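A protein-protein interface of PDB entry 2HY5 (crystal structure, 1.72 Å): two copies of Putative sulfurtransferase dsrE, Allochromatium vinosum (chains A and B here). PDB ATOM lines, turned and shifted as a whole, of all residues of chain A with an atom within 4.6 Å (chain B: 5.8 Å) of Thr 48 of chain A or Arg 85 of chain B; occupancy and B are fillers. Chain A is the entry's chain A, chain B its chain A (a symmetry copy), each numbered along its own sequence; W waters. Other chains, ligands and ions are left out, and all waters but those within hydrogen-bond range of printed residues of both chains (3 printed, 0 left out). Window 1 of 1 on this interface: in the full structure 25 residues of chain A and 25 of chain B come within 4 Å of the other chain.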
ATOM      1  N   GLN A  13      28.048  11.560 -28.130  1.00  0.00           N
ATOM      2  CA  GLN A  13      28.109  10.226 -28.734  1.00  0.00           C
ATOM      3  C   GLN A  13      28.162  10.316 -30.257  1.00  0.00           C
ATOM      4  O   GLN A  13      28.906   9.587 -30.901  1.00  0.00           O
ATOM      5  CB  GLN A  13      26.894   9.394 -28.315  1.00  0.00           C
ATOM      6  CG  GLN A  13      26.935   7.940 -28.801  1.00  0.00           C
ATOM      7  CD  GLN A  13      27.613   6.997 -27.822  1.00  0.00           C
ATOM      8  OE1 GLN A  13      28.228   7.424 -26.843  1.00  0.00           O
ATOM      9  NE2 GLN A  13      27.498   5.699 -28.082  1.00  0.00           N
ATOM     10  N   ASN A  45      18.311  13.640 -25.014  1.00  0.00           N
ATOM     11  CA  ASN A  45      19.367  13.760 -24.016  1.00  0.00           C
ATOM     12  C   ASN A  45      20.175  15.060 -24.118  1.00  0.00           C
ATOM     13  O   ASN A  45      21.060  15.316 -23.299  1.00  0.00           O
ATOM     14  CB  ASN A  45      20.287  12.532 -24.089  1.00  0.00           C
ATOM     15  CG  ASN A  45      19.593  11.253 -23.615  1.00  0.00           C
ATOM     16  OD1 ASN A  45      19.988  10.143 -23.982  1.00  0.00           O
ATOM     17  ND2 ASN A  45      18.563  11.407 -22.789  1.00  0.00           N
ATOM     18  N   ASN A  46      19.863  15.880 -25.120  1.00  0.00           N
ATOM     19  CA  ASN A  46      20.540  17.164 -25.292  1.00  0.00           C
ATOM     20  C   ASN A  46      19.898  18.205 -24.387  1.00  0.00           C
ATOM     21  O   ASN A  46      20.323  19.360 -24.367  1.00  0.00           O
ATOM     22  CB  ASN A  46      20.400  17.663 -26.729  1.00  0.00           C
ATOM     23  CG  ASN A  46      21.335  16.968 -27.678  1.00  0.00           C
ATOM     24  OD1 ASN A  46      22.535  17.227 -27.680  1.00  0.00           O
ATOM     25  ND2 ASN A  46      20.791  16.073 -28.493  1.00  0.00           N
ATOM     26  N   SER A  47      18.884  17.793 -23.634  1.00  0.00           N
ATOM     27  CA  SER A  47      18.163  18.734 -22.784  1.00  0.00           C
ATOM     28  C   SER A  47      18.385  18.612 -21.282  1.00  0.00           C
ATOM     29  O   SER A  47      17.728  19.307 -20.508  1.00  0.00           O
ATOM     30  CB  SER A  47      16.665  18.631 -23.064  1.00  0.00           C
ATOM     31  OG  SER A  47      16.147  17.387 -22.633  1.00  0.00           O
ATOM     32  N   THR A  48      19.293  17.740 -20.860  1.00  0.00           N
ATOM     33  CA  THR A  48      19.548  17.583 -19.432  1.00  0.00           C
ATOM     34  C   THR A  48      20.499  18.654 -18.912  1.00  0.00           C
ATOM     35  O   THR A  48      21.455  19.025 -19.588  1.00  0.00           O
ATOM     36  CB  THR A  48      20.140  16.192 -19.108  1.00  0.00           C
ATOM     37  OG1 THR A  48      20.546  16.159 -17.734  1.00  0.00           O
ATOM     38  CG2 THR A  48      21.333  15.890 -19.994  1.00  0.00           C
ATOM     39  N   ARG A  49      20.235  19.139 -17.703  1.00  0.00           N
ATOM     40  CA  ARG A  49      21.064  20.172 -17.083  1.00  0.00           C
ATOM     41  C   ARG A  49      22.128  19.553 -16.181  1.00  0.00           C
ATOM     42  O   ARG A  49      22.897  20.266 -15.543  1.00  0.00           O
ATOM     43  CB  ARG A  49      20.195  21.119 -16.244  1.00  0.00           C
ATOM     44  CG  ARG A  49      19.590  20.483 -14.983  1.00  0.00           C
ATOM     45  CD  ARG A  49      18.839  21.525 -14.135  1.00  0.00           C
ATOM     46  NE  ARG A  49      18.415  20.997 -12.836  1.00  0.00           N
ATOM     47  CZ  ARG A  49      17.289  20.319 -12.630  1.00  0.00           C
ATOM     48  NH1 ARG A  49      16.458  20.084 -13.638  1.00  0.00           N
ATOM     49  NH2 ARG A  49      16.991  19.872 -11.412  1.00  0.00           N
ATOM     50  N   LEU A  50      22.183  18.225 -16.152  1.00  0.00           N
ATOM     51  CA  LEU A  50      23.125  17.529 -15.291  1.00  0.00           C
ATOM     52  C   LEU A  50      24.492  17.186 -15.882  1.00  0.00           C
ATOM     53  O   LEU A  50      25.259  16.455 -15.258  1.00  0.00           O
ATOM     54  CB  LEU A  50      22.472  16.256 -14.739  1.00  0.00           C
ATOM     55  CG  LEU A  50      21.186  16.455 -13.930  1.00  0.00           C
ATOM     56  CD1 LEU A  50      20.668  15.098 -13.456  1.00  0.00           C
ATOM     57  CD2 LEU A  50      21.450  17.378 -12.733  1.00  0.00           C
ATOM     58  N   THR A  51      24.814  17.710 -17.062  1.00  0.00           N
ATOM     59  CA  THR A  51      26.122  17.408 -17.645  1.00  0.00           C
ATOM     60  C   THR A  51      27.240  18.298 -17.096  1.00  0.00           C
ATOM     61  O   THR A  51      27.028  19.463 -16.767  1.00  0.00           O
ATOM     62  CB  THR A  51      26.123  17.525 -19.196  1.00  0.00           C
ATOM     63  OG1 THR A  51      26.055  18.900 -19.590  1.00  0.00           O
ATOM     64  CG2 THR A  51      24.940  16.770 -19.789  1.00  0.00           C
ATOM     65  N   VAL A  61      24.942  21.259 -24.140  1.00  0.00           N
ATOM     66  CA  VAL A  61      23.673  21.707 -23.591  1.00  0.00           C
ATOM     67  C   VAL A  61      23.633  23.210 -23.356  1.00  0.00           C
ATOM     68  O   VAL A  61      22.689  23.874 -23.781  1.00  0.00           O
ATOM     69  CB  VAL A  61      23.344  20.984 -22.275  1.00  0.00           C
ATOM     70  CG1 VAL A  61      21.977  21.440 -21.756  1.00  0.00           C
ATOM     71  CG2 VAL A  61      23.347  19.476 -22.508  1.00  0.00           C
ATOM     72  N   ILE A  87      14.315  11.857 -19.196  1.00  0.00           N
ATOM     73  CA  ILE A  87      14.374  13.318 -19.206  1.00  0.00           C
ATOM     74  C   ILE A  87      13.076  13.711 -18.516  1.00  0.00           C
ATOM     75  O   ILE A  87      11.985  13.368 -18.982  1.00  0.00           O
ATOM     76  CB  ILE A  87      14.422  13.894 -20.639  1.00  0.00           C
ATOM     77  CG1 ILE A  87      15.755  13.529 -21.301  1.00  0.00           C
ATOM     78  CG2 ILE A  87      14.270  15.414 -20.594  1.00  0.00           C
ATOM     79  CD1 ILE A  87      16.986  14.122 -20.618  1.00  0.00           C
ATOM     80  N   ASN A 102      15.569  16.727 -14.241  1.00  0.00           N
ATOM     81  CA  ASN A 102      16.885  16.944 -14.820  1.00  0.00           C
ATOM     82  C   ASN A 102      16.864  17.795 -16.082  1.00  0.00           C
ATOM     83  O   ASN A 102      17.906  18.077 -16.662  1.00  0.00           O
ATOM     84  CB  ASN A 102      17.567  15.600 -15.105  1.00  0.00           C
ATOM     85  CG  ASN A 102      16.854  14.801 -16.172  1.00  0.00           C
ATOM     86  OD1 ASN A 102      15.678  15.026 -16.445  1.00  0.00           O
ATOM     87  ND2 ASN A 102      17.561  13.852 -16.775  1.00  0.00           N
ATOM     88  N   ILE A 103      15.686  18.235 -16.500  1.00  0.00           N
ATOM     89  CA  ILE A 103      15.628  19.044 -17.711  1.00  0.00           C
ATOM     90  C   ILE A 103      16.235  20.434 -17.521  1.00  0.00           C
ATOM     91  O   ILE A 103      16.187  21.012 -16.431  1.00  0.00           O
ATOM     92  CB  ILE A 103      14.181  19.202 -18.221  1.00  0.00           C
ATOM     93  CG1 ILE A 103      14.209  19.643 -19.686  1.00  0.00           C
ATOM     94  CG2 ILE A 103      13.423  20.224 -17.375  1.00  0.00           C
ATOM     95  CD1 ILE A 103      12.853  19.972 -20.247  1.00  0.00           C
ATOM     96  N   HIS A 104      16.841  20.952 -18.582  1.00  0.00           N
ATOM     97  CA  HIS A 104      17.422  22.287 -18.549  1.00  0.00           C
ATOM     98  C   HIS A 104      16.224  23.220 -18.763  1.00  0.00           C
ATOM     99  O   HIS A 104      15.410  23.000 -19.661  1.00  0.00           O
ATOM    100  CB  HIS A 104      18.451  22.430 -19.678  1.00  0.00           C
ATOM    101  CG  HIS A 104      19.185  23.734 -19.667  1.00  0.00           C
ATOM    102  ND1 HIS A 104      18.573  24.936 -19.950  1.00  0.00           N
ATOM    103  CD2 HIS A 104      20.482  24.026 -19.400  1.00  0.00           C
ATOM    104  CE1 HIS A 104      19.458  25.912 -19.858  1.00  0.00           C
ATOM    105  NE2 HIS A 104      20.625  25.387 -19.525  1.00  0.00           N
ATOM    106  N   HIS B  41      30.574   4.958 -22.609  1.00  0.00           N
ATOM    107  CA  HIS B  41      29.951   5.732 -23.691  1.00  0.00           C
ATOM    108  C   HIS B  41      28.494   5.990 -23.281  1.00  0.00           C
ATOM    109  O   HIS B  41      28.207   6.179 -22.100  1.00  0.00           O
ATOM    110  CB  HIS B  41      29.980   4.960 -25.018  1.00  0.00           C
ATOM    111  CG  HIS B  41      31.345   4.518 -25.450  1.00  0.00           C
ATOM    112  ND1 HIS B  41      32.376   5.399 -25.701  1.00  0.00           N
ATOM    113  CD2 HIS B  41      31.836   3.284 -25.721  1.00  0.00           C
ATOM    114  CE1 HIS B  41      33.439   4.730 -26.107  1.00  0.00           C
ATOM    115  NE2 HIS B  41      33.137   3.443 -26.129  1.00  0.00           N
ATOM    116  N   ASP B  42      27.577   5.993 -24.247  1.00  0.00           N
ATOM    117  CA  ASP B  42      26.157   6.206 -23.951  1.00  0.00           C
ATOM    118  C   ASP B  42      25.612   5.099 -23.051  1.00  0.00           C
ATOM    119  O   ASP B  42      24.490   5.185 -22.555  1.00  0.00           O
ATOM    120  CB  ASP B  42      25.337   6.258 -25.243  1.00  0.00           C
ATOM    121  CG  ASP B  42      25.195   7.664 -25.794  1.00  0.00           C
ATOM    122  OD1 ASP B  42      25.770   8.603 -25.200  1.00  0.00           O
ATOM    123  OD2 ASP B  42      24.505   7.828 -26.824  1.00  0.00           O
ATOM    124  N   GLY B  43      26.414   4.059 -22.847  1.00  0.00           N
ATOM    125  CA  GLY B  43      26.001   2.963 -21.993  1.00  0.00           C
ATOM    126  C   GLY B  43      25.693   3.436 -20.584  1.00  0.00           C
ATOM    127  O   GLY B  43      24.890   2.823 -19.882  1.00  0.00           O
ATOM    128  N   VAL B  44      26.320   4.528 -20.160  1.00  0.00           N
ATOM    129  CA  VAL B  44      26.075   5.036 -18.814  1.00  0.00           C
ATOM    130  C   VAL B  44      24.606   5.402 -18.592  1.00  0.00           C
ATOM    131  O   VAL B  44      24.137   5.442 -17.452  1.00  0.00           O
ATOM    132  CB  VAL B  44      26.957   6.278 -18.503  1.00  0.00           C
ATOM    133  CG1 VAL B  44      28.433   5.905 -18.621  1.00  0.00           C
ATOM    134  CG2 VAL B  44      26.610   7.418 -19.450  1.00  0.00           C
ATOM    135  N   ASN B  45      23.874   5.643 -19.677  1.00  0.00           N
ATOM    136  CA  ASN B  45      22.469   6.019 -19.568  1.00  0.00           C
ATOM    137  C   ASN B  45      21.552   4.876 -19.118  1.00  0.00           C
ATOM    138  O   ASN B  45      20.349   5.071 -18.929  1.00  0.00           O
ATOM    139  CB  ASN B  45      21.991   6.617 -20.900  1.00  0.00           C
ATOM    140  CG  ASN B  45      22.628   7.978 -21.191  1.00  0.00           C
ATOM    141  OD1 ASN B  45      22.711   8.406 -22.345  1.00  0.00           O
ATOM    142  ND2 ASN B  45      23.067   8.665 -20.142  1.00  0.00           N
ATOM    143  N   ALA B  80      33.740   9.549 -16.122  1.00  0.00           N
ATOM    144  CA  ALA B  80      34.041  10.481 -17.208  1.00  0.00           C
ATOM    145  C   ALA B  80      32.890  10.548 -18.201  1.00  0.00           C
ATOM    146  O   ALA B  80      32.426  11.632 -18.566  1.00  0.00           O
ATOM    147  CB  ALA B  80      35.320  10.054 -17.919  1.00  0.00           C
ATOM    148  N   ALA B  81      32.432   9.381 -18.637  1.00  0.00           N
ATOM    149  CA  ALA B  81      31.326   9.298 -19.579  1.00  0.00           C
ATOM    150  C   ALA B  81      30.030   9.796 -18.931  1.00  0.00           C
ATOM    151  O   ALA B  81      29.184  10.389 -19.594  1.00  0.00           O
ATOM    152  CB  ALA B  81      31.161   7.856 -20.062  1.00  0.00           C
ATOM    153  N   ALA B  82      29.880   9.559 -17.630  1.00  0.00           N
ATOM    154  CA  ALA B  82      28.686  10.004 -16.912  1.00  0.00           C
ATOM    155  C   ALA B  82      28.628  11.530 -16.790  1.00  0.00           C
ATOM    156  O   ALA B  82      27.563  12.130 -16.923  1.00  0.00           O
ATOM    157  CB  ALA B  82      28.644   9.370 -15.525  1.00  0.00           C
ATOM    158  N   GLN B  83      29.775  12.156 -16.538  1.00  0.00           N
ATOM    159  CA  GLN B  83      29.831  13.608 -16.404  1.00  0.00           C
ATOM    160  C   GLN B  83      29.488  14.291 -17.717  1.00  0.00           C
ATOM    161  O   GLN B  83      28.848  15.335 -17.742  1.00  0.00           O
ATOM    162  CB  GLN B  83      31.223  14.044 -15.946  1.00  0.00           C
ATOM    163  CG  GLN B  83      31.531  13.667 -14.511  1.00  0.00           C
ATOM    164  CD  GLN B  83      32.952  13.997 -14.113  1.00  0.00           C
ATOM    165  OE1 GLN B  83      33.312  13.924 -12.937  1.00  0.00           O
ATOM    166  NE2 GLN B  83      33.773  14.355 -15.092  1.00  0.00           N
ATOM    167  N   ARG B  84      29.916  13.684 -18.812  1.00  0.00           N
ATOM    168  CA  ARG B  84      29.662  14.237 -20.128  1.00  0.00           C
ATOM    169  C   ARG B  84      28.183  14.132 -20.491  1.00  0.00           C
ATOM    170  O   ARG B  84      27.628  15.016 -21.145  1.00  0.00           O
ATOM    171  CB  ARG B  84      30.496  13.478 -21.159  1.00  0.00           C
ATOM    172  CG  ARG B  84      30.910  14.271 -22.381  1.00  0.00           C
ATOM    173  CD  ARG B  84      31.818  13.413 -23.246  1.00  0.00           C
ATOM    174  NE  ARG B  84      32.798  12.699 -22.430  1.00  0.00           N
ATOM    175  CZ  ARG B  84      34.082  13.030 -22.321  1.00  0.00           C
ATOM    176  NH1 ARG B  84      34.563  14.073 -22.984  1.00  0.00           N
ATOM    177  NH2 ARG B  84      34.883  12.320 -21.539  1.00  0.00           N
ATOM    178  N   ARG B  85      27.537  13.067 -20.030  1.00  0.00           N
ATOM    179  CA  ARG B  85      26.146  12.816 -20.374  1.00  0.00           C
ATOM    180  C   ARG B  85      25.054  13.146 -19.363  1.00  0.00           C
ATOM    181  O   ARG B  85      23.870  13.136 -19.707  1.00  0.00           O
ATOM    182  CB  ARG B  85      26.029  11.366 -20.830  1.00  0.00           C
ATOM    183  CG  ARG B  85      26.939  11.068 -22.022  1.00  0.00           C
ATOM    184  CD  ARG B  85      26.941   9.600 -22.376  1.00  0.00           C
ATOM    185  NE  ARG B  85      27.672   9.319 -23.612  1.00  0.00           N
ATOM    186  CZ  ARG B  85      28.994   9.361 -23.746  1.00  0.00           C
ATOM    187  NH1 ARG B  85      29.766   9.680 -22.719  1.00  0.00           N
ATOM    188  NH2 ARG B  85      29.549   9.047 -24.914  1.00  0.00           N
ATOM    189  N   GLY B  86      25.432  13.429 -18.124  1.00  0.00           N
ATOM    190  CA  GLY B  86      24.425  13.780 -17.142  1.00  0.00           C
ATOM    191  C   GLY B  86      23.965  12.705 -16.176  1.00  0.00           C
ATOM    192  O   GLY B  86      22.812  12.729 -15.755  1.00  0.00           O
ATOM    193  N   ILE B  87      24.830  11.755 -15.841  1.00  0.00           N
ATOM    194  CA  ILE B  87      24.468  10.726 -14.867  1.00  0.00           C
ATOM    195  C   ILE B  87      25.149  11.213 -13.596  1.00  0.00           C
ATOM    196  O   ILE B  87      26.374  11.365 -13.555  1.00  0.00           O
ATOM    197  CB  ILE B  87      24.996   9.329 -15.264  1.00  0.00           C
ATOM    198  CG1 ILE B  87      24.266   8.836 -16.517  1.00  0.00           C
ATOM    199  CG2 ILE B  87      24.774   8.344 -14.118  1.00  0.00           C
ATOM    200  CD1 ILE B  87      22.763   8.630 -16.337  1.00  0.00           C
ATOM    201  N   ASN B 102      20.311  11.537 -10.421  1.00  0.00           N
ATOM    202  CA  ASN B 102      19.429  10.702 -11.220  1.00  0.00           C
ATOM    203  C   ASN B 102      19.873   9.248 -11.303  1.00  0.00           C
ATOM    204  O   ASN B 102      19.209   8.428 -11.925  1.00  0.00           O
ATOM    205  CB  ASN B 102      19.281  11.286 -12.631  1.00  0.00           C
ATOM    206  CG  ASN B 102      20.575  11.257 -13.411  1.00  0.00           C
ATOM    207  OD1 ASN B 102      21.655  11.168 -12.833  1.00  0.00           O
ATOM    208  ND2 ASN B 102      20.474  11.343 -14.733  1.00  0.00           N
HETATM  209  O   HOH W   1      23.226  13.803 -22.193  1.00  0.00           O
HETATM  210  O   HOH W   2      20.497  13.628 -17.099  1.00  0.00           O
HETATM  211  O   HOH W   3      18.191  10.636 -16.483  1.00  0.00           O
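Water W2 lies within hydrogen-bond range of the side-chain hydroxyl of Thr 48 of chain A (2.6 Å), the backbone carbonyl oxygen of Gly 86 of chain B (2.8 Å), the side-chain amide nitrogen of Asn 102 of chain A (3.0 Å) and the side-chain amide nitrogen of Asn 102 of chain B (3.3 Å).
Water W1 bridges the backbone carbonyl oxygen of Arg 85 of chain B and the backbone carbonyl oxygen of Asn 45 of chain A.
Water W3 lies within hydrogen-bond range of the side-chain amide nitrogen of Asn 102 of chain B (3.0 Å) and the side-chain amide nitrogen of Asn 102 of chain A (3.3 Å).
OG1 of Thr 48 of chain A lies within hydrogen-bond range of N of Leu 50 of chain A.
The backbone carbonyl oxygen (O) of Asn 102 of chain A lies close to the side-chain hydroxyl (OG1) of Thr 48 of chain A, at 3.4 Å.
The side-chain carboxylate (OD1) of Asp 42 of chain B lies within salt-bridge range of the guanidinium group (NE) of Arg 85 of chain B (2.6 Å).
O of Ala 81 of chain B sits at hydrogen-bond distance from NH1 of Arg 85 of chain B, at 3.3 Å.
ND2 of Asn 102 of chain B sits at hydrogen-bond distance from O of Gly 86 of chain B (2.9 Å).
Of the 14 printed residues of chain B, 8 touch a printed residue of chain A.
Printed residues of chain B that touch a printed residue of chain A: His 41, Asp 42, Asn 45, Gln 83, Arg 84, Arg 85, Gly 86 and Asn 102.
Hydrophobic or aromatic side chains of chain B within 4 Å of the printed part of chain A: His 41.
Of the 13 printed residues of chain A, 5 touch a printed residue of chain B.
Hydrophobic or aromatic side chains of chain A that line the printed part of chain B: Leu 50.
Among the printed residues, 11 pairs touch across the chains.
Among the printed residues, no Asp or Glu carboxylate lies within 4 Å of a Lys or Arg side-chain nitrogen of the other chain.
Among the printed residues, pairs that only touch across the chains: Gln 13 of chain A with His 41 of chain B (3.5 Å), Asn 45 of chain A with Asn 45 of chain B (3.6 Å), Thr 48 of chain A with Arg 85 of chain B (3.8 Å), Leu 50 of chain A with Gly 86 of chain B (3.4 Å), Leu 50 of chain A with Asn 102 of chain B (3.8 Å), Thr 51 of chain A with Gln 83 of chain B (3.4 Å), Thr 51 of chain A with Arg 84 of chain B (3.5 Å), Thr 51 of chain A with Arg 85 of chain B (3.7 Å) and Thr 51 of chain A with Gly 86 of chain B (3.8 Å).
Of chain B, only Arg 85 (3.8 Å) comes within 4 Å of Thr 48 of chain A.
Arg 49 of chain A touches none of the printed residues of chain B.
Printed residues of chain B within 4 Å of Leu 50 of chain A: Gly 86 and Asn 102.
Of the printed residues of chain A, Asp 42 of chain B touches Gln 13 (3.0 Å).
Ala 81 of chain B touches none of the printed residues of chain A.
Of the printed residues of chain A, Arg 84 of chain B touches Thr 51 (3.5 Å).
Of chain A, only Gln 13 (2.8 Å), Thr 48 (3.8 Å) and Thr 51 (3.7 Å) come within 4 Å of Arg 85 of chain B.
The nearest printed residue of chain A that does not touch Arg 84 of chain B is Val 61 of chain A (6.3 Å).
The backbone NH (N) of Asp 42 of chain B sits at hydrogen-bond distance from the side-chain amide oxygen (OE1) of Gln 13 of chain A, at 3.0 Å.
OE1 of Gln 13 of chain A is in hydrogen-bond range of NH2 of Arg 85 of chain B (2.8 Å).
Asn 45 of chain B touches its own counterpart, Asn 45 of chain A.
Positions printed for both chains: 45, 87 and 102.
Of the 11 pairs that touch across the chains among the printed residues, 1 has its exchanged pair printed and touching as well.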
